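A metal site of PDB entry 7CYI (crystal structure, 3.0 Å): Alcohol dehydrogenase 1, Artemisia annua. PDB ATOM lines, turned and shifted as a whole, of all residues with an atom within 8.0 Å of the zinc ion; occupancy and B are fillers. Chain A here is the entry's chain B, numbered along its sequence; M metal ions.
Merely in contact with the zinc ion: Gly 100 and His 114.
The zinc ion is bound by the side-chain sulfur (SG) of Cys 113. The side-chain sulfur (SG) of Cys 102 is bound to the zinc ion (2.4 Å). The zinc ion is bound by SG of Cys 99 (2.5 Å). The side-chain sulfur (SG) of Cys 105 is bound to the zinc ion, at 2.5 Å. The zinc ion has four donor atoms within binding distance.
SG of Cys 99 sits close to N of Gln 101 (3.4 Å). The side-chain sulfur of Cys 113 sits close to the backbone NH of Val 115 (3.0 Å). The backbone NH (N) of Asn 104 lies close to the side-chain sulfur (SG) of Cys 102. The side-chain sulfur of Cys 105 sits close to the backbone NH of Gly 100 (3.4 Å). The side-chain sulfur of Cys 113 sits close to the backbone NH of Tyr 116, 3.3 Å away. OD1 of Asn 104 sits at hydrogen-bond distance from NE2 of His 114 (3.0 Å). The side-chain sulfur of Cys 102 sits close to the backbone NH of His 114, at 3.3 Å.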
ATOM      1  N   GLY A  97     -10.763 -21.837 -17.068  1.00  0.00           N
ATOM      2  CA  GLY A  97     -10.563 -22.901 -18.013  1.00  0.00           C
ATOM      3  C   GLY A  97     -10.266 -24.241 -17.350  1.00  0.00           C
ATOM      4  O   GLY A  97     -10.201 -24.371 -16.128  1.00  0.00           O
ATOM      5  N   GLU A  98     -10.099 -25.256 -18.198  1.00  0.00           N
ATOM      6  CA  GLU A  98      -9.721 -26.598 -17.751  1.00  0.00           C
ATOM      7  C   GLU A  98      -8.787 -27.183 -18.811  1.00  0.00           C
ATOM      8  O   GLU A  98      -9.252 -27.695 -19.829  1.00  0.00           O
ATOM      9  CB  GLU A  98     -10.943 -27.479 -17.538  1.00  0.00           C
ATOM     10  CG  GLU A  98     -10.601 -28.882 -17.057  1.00  0.00           C
ATOM     11  CD  GLU A  98     -11.804 -29.801 -17.047  1.00  0.00           C
ATOM     12  OE1 GLU A  98     -12.887 -29.375 -17.509  1.00  0.00           O
ATOM     13  OE2 GLU A  98     -11.668 -30.948 -16.579  1.00  0.00           O
ATOM     14  N   CYS A  99      -7.485 -27.114 -18.554  1.00  0.00           N
ATOM     15  CA  CYS A  99      -6.486 -27.600 -19.505  1.00  0.00           C
ATOM     16  C   CYS A  99      -6.547 -29.119 -19.603  1.00  0.00           C
ATOM     17  O   CYS A  99      -6.969 -29.664 -20.626  1.00  0.00           O
ATOM     18  CB  CYS A  99      -5.086 -27.133 -19.097  1.00  0.00           C
ATOM     19  SG  CYS A  99      -4.378 -27.986 -17.674  1.00  0.00           S
ATOM     20  N   GLY A 100      -6.125 -29.809 -18.549  1.00  0.00           N
ATOM     21  CA  GLY A 100      -6.178 -31.253 -18.520  1.00  0.00           C
ATOM     22  C   GLY A 100      -4.926 -31.915 -17.998  1.00  0.00           C
ATOM     23  O   GLY A 100      -4.987 -33.026 -17.455  1.00  0.00           O
ATOM     24  N   GLN A 101      -3.776 -31.253 -18.143  1.00  0.00           N
ATOM     25  CA  GLN A 101      -2.498 -31.847 -17.769  1.00  0.00           C
ATOM     26  C   GLN A 101      -1.790 -31.125 -16.627  1.00  0.00           C
ATOM     27  O   GLN A 101      -0.744 -31.605 -16.180  1.00  0.00           O
ATOM     28  CB  GLN A 101      -1.571 -31.910 -18.981  1.00  0.00           C
ATOM     29  CG  GLN A 101      -1.844 -33.077 -19.914  1.00  0.00           C
ATOM     30  CD  GLN A 101      -3.081 -32.853 -20.765  1.00  0.00           C
ATOM     31  OE1 GLN A 101      -3.409 -31.706 -21.109  1.00  0.00           O
ATOM     32  NE2 GLN A 101      -3.784 -33.927 -21.090  1.00  0.00           N
ATOM     33  N   CYS A 102      -2.314 -30.004 -16.152  1.00  0.00           N
ATOM     34  CA  CYS A 102      -1.715 -29.376 -14.986  1.00  0.00           C
ATOM     35  C   CYS A 102      -1.974 -30.224 -13.740  1.00  0.00           C
ATOM     36  O   CYS A 102      -2.872 -31.071 -13.708  1.00  0.00           O
ATOM     37  CB  CYS A 102      -2.250 -27.954 -14.790  1.00  0.00           C
ATOM     38  SG  CYS A 102      -3.908 -27.826 -14.097  1.00  0.00           S
ATOM     39  N   LEU A 103      -1.173 -29.992 -12.702  1.00  0.00           N
ATOM     40  CA  LEU A 103      -1.200 -30.855 -11.529  1.00  0.00           C
ATOM     41  C   LEU A 103      -2.542 -30.855 -10.818  1.00  0.00           C
ATOM     42  O   LEU A 103      -2.862 -31.815 -10.105  1.00  0.00           O
ATOM     43  CB  LEU A 103      -0.090 -30.453 -10.555  1.00  0.00           C
ATOM     44  CG  LEU A 103       1.334 -30.796 -10.997  1.00  0.00           C
ATOM     45  CD1 LEU A 103       2.348 -30.374  -9.936  1.00  0.00           C
ATOM     46  CD2 LEU A 103       1.447 -32.280 -11.291  1.00  0.00           C
ATOM     47  N   ASN A 104      -3.346 -29.798 -10.988  1.00  0.00           N
ATOM     48  CA  ASN A 104      -4.595 -29.701 -10.238  1.00  0.00           C
ATOM     49  C   ASN A 104      -5.700 -30.537 -10.861  1.00  0.00           C
ATOM     50  O   ASN A 104      -6.191 -31.495 -10.249  1.00  0.00           O
ATOM     51  CB  ASN A 104      -5.024 -28.237 -10.122  1.00  0.00           C
ATOM     52  CG  ASN A 104      -4.911 -27.709  -8.704  1.00  0.00           C
ATOM     53  OD1 ASN A 104      -4.034 -28.122  -7.948  1.00  0.00           O
ATOM     54  ND2 ASN A 104      -5.799 -26.788  -8.345  1.00  0.00           N
ATOM     55  N   CYS A 105      -6.120 -30.196 -12.082  1.00  0.00           N
ATOM     56  CA  CYS A 105      -7.196 -30.942 -12.726  1.00  0.00           C
ATOM     57  C   CYS A 105      -6.775 -32.349 -13.133  1.00  0.00           C
ATOM     58  O   CYS A 105      -7.635 -33.126 -13.567  1.00  0.00           O
ATOM     59  CB  CYS A 105      -7.725 -30.174 -13.941  1.00  0.00           C
ATOM     60  SG  CYS A 105      -6.491 -29.807 -15.191  1.00  0.00           S
ATOM     61  N   LYS A 106      -5.495 -32.690 -13.001  1.00  0.00           N
ATOM     62  CA  LYS A 106      -5.073 -34.078 -13.161  1.00  0.00           C
ATOM     63  C   LYS A 106      -5.551 -34.960 -12.024  1.00  0.00           C
ATOM     64  O   LYS A 106      -5.607 -36.184 -12.181  1.00  0.00           O
ATOM     65  CB  LYS A 106      -3.546 -34.146 -13.281  1.00  0.00           C
ATOM     66  CG  LYS A 106      -3.000 -35.460 -13.816  1.00  0.00           C
ATOM     67  CD  LYS A 106      -1.471 -35.458 -13.852  1.00  0.00           C
ATOM     68  CE  LYS A 106      -0.887 -35.697 -12.468  1.00  0.00           C
ATOM     69  NZ  LYS A 106       0.588 -35.510 -12.408  1.00  0.00           N
ATOM     70  N   THR A 110     -10.764 -30.703  -8.222  1.00  0.00           N
ATOM     71  CA  THR A 110     -10.888 -29.254  -8.239  1.00  0.00           C
ATOM     72  C   THR A 110     -11.126 -28.791  -9.671  1.00  0.00           C
ATOM     73  O   THR A 110     -10.814 -29.488 -10.634  1.00  0.00           O
ATOM     74  CB  THR A 110      -9.633 -28.571  -7.671  1.00  0.00           C
ATOM     75  OG1 THR A 110      -9.889 -27.168  -7.517  1.00  0.00           O
ATOM     76  CG2 THR A 110      -8.449 -28.760  -8.593  1.00  0.00           C
ATOM     77  N   ASN A 111     -11.707 -27.603  -9.787  1.00  0.00           N
ATOM     78  CA  ASN A 111     -11.941 -26.960 -11.071  1.00  0.00           C
ATOM     79  C   ASN A 111     -11.006 -25.780 -11.309  1.00  0.00           C
ATOM     80  O   ASN A 111     -11.103 -25.131 -12.359  1.00  0.00           O
ATOM     81  CB  ASN A 111     -13.392 -26.505 -11.184  1.00  0.00           C
ATOM     82  CG  ASN A 111     -13.758 -25.461 -10.156  1.00  0.00           C
ATOM     83  OD1 ASN A 111     -13.144 -25.368  -9.098  1.00  0.00           O
ATOM     84  ND2 ASN A 111     -14.770 -24.653 -10.468  1.00  0.00           N
ATOM     85  N   LEU A 112     -10.125 -25.480 -10.360  1.00  0.00           N
ATOM     86  CA  LEU A 112      -9.205 -24.345 -10.477  1.00  0.00           C
ATOM     87  C   LEU A 112      -7.963 -24.829 -11.217  1.00  0.00           C
ATOM     88  O   LEU A 112      -6.993 -25.291 -10.612  1.00  0.00           O
ATOM     89  CB  LEU A 112      -8.862 -23.792  -9.097  1.00  0.00           C
ATOM     90  CG  LEU A 112     -10.079 -23.420  -8.242  1.00  0.00           C
ATOM     91  CD1 LEU A 112      -9.686 -23.236  -6.793  1.00  0.00           C
ATOM     92  CD2 LEU A 112     -10.731 -22.157  -8.787  1.00  0.00           C
ATOM     93  N   CYS A 113      -7.991 -24.715 -12.537  1.00  0.00           N
ATOM     94  CA  CYS A 113      -6.871 -25.142 -13.354  1.00  0.00           C
ATOM     95  C   CYS A 113      -5.694 -24.192 -13.203  1.00  0.00           C
ATOM     96  O   CYS A 113      -5.867 -22.965 -13.136  1.00  0.00           O
ATOM     97  CB  CYS A 113      -7.283 -25.231 -14.826  1.00  0.00           C
ATOM     98  SG  CYS A 113      -5.918 -25.154 -16.004  1.00  0.00           S
ATOM     99  N   HIS A 114      -4.487 -24.758 -13.158  1.00  0.00           N
ATOM    100  CA  HIS A 114      -3.289 -23.943 -13.004  1.00  0.00           C
ATOM    101  C   HIS A 114      -2.992 -23.138 -14.262  1.00  0.00           C
ATOM    102  O   HIS A 114      -2.430 -22.041 -14.185  1.00  0.00           O
ATOM    103  CB  HIS A 114      -2.081 -24.832 -12.667  1.00  0.00           C
ATOM    104  CG  HIS A 114      -2.125 -25.404 -11.284  1.00  0.00           C
ATOM    105  ND1 HIS A 114      -1.363 -26.486 -10.911  1.00  0.00           N
ATOM    106  CD2 HIS A 114      -2.822 -25.031 -10.189  1.00  0.00           C
ATOM    107  CE1 HIS A 114      -1.597 -26.762  -9.640  1.00  0.00           C
ATOM    108  NE2 HIS A 114      -2.474 -25.888  -9.174  1.00  0.00           N
ATOM    109  N   VAL A 115      -3.361 -23.665 -15.431  1.00  0.00           N
ATOM    110  CA  VAL A 115      -2.957 -23.044 -16.697  1.00  0.00           C
ATOM    111  C   VAL A 115      -3.894 -21.901 -17.079  1.00  0.00           C
ATOM    112  O   VAL A 115      -3.463 -20.886 -17.631  1.00  0.00           O
ATOM    113  CB  VAL A 115      -2.876 -24.110 -17.796  1.00  0.00           C
ATOM    114  CG1 VAL A 115      -2.247 -23.538 -19.050  1.00  0.00           C
ATOM    115  CG2 VAL A 115      -2.094 -25.314 -17.301  1.00  0.00           C
ATOM    116  N   TYR A 116      -5.190 -22.045 -16.783  1.00  0.00           N
ATOM    117  CA  TYR A 116      -6.198 -21.057 -17.167  1.00  0.00           C
ATOM    118  C   TYR A 116      -6.932 -20.553 -15.920  1.00  0.00           C
ATOM    119  O   TYR A 116      -8.100 -20.912 -15.693  1.00  0.00           O
ATOM    120  CB  TYR A 116      -7.179 -21.639 -18.183  1.00  0.00           C
ATOM    121  CG  TYR A 116      -6.491 -22.226 -19.397  1.00  0.00           C
ATOM    122  CD1 TYR A 116      -5.432 -21.569 -20.013  1.00  0.00           C
ATOM    123  CD2 TYR A 116      -6.908 -23.436 -19.933  1.00  0.00           C
ATOM    124  CE1 TYR A 116      -4.803 -22.104 -21.117  1.00  0.00           C
ATOM    125  CE2 TYR A 116      -6.284 -23.982 -21.044  1.00  0.00           C
ATOM    126  CZ  TYR A 116      -5.238 -23.307 -21.626  1.00  0.00           C
ATOM    127  OH  TYR A 116      -4.609 -23.842 -22.730  1.00  0.00           O
ATOM    128  N   PRO A 117      -6.283 -19.722 -15.114  1.00  0.00           N
ATOM    129  CA  PRO A 117      -6.941 -19.184 -13.927  1.00  0.00           C
ATOM    130  C   PRO A 117      -7.861 -18.031 -14.294  1.00  0.00           C
ATOM    131  O   PRO A 117      -7.811 -17.528 -15.435  1.00  0.00           O
ATOM    132  CB  PRO A 117      -5.763 -18.690 -13.070  1.00  0.00           C
ATOM    133  CG  PRO A 117      -4.754 -18.273 -14.084  1.00  0.00           C
ATOM    134  CD  PRO A 117      -4.917 -19.213 -15.261  1.00  0.00           C
HETATM  135 ZN    ZN M   1      -5.723 -27.466 -15.679  1.00  0.00          ZN
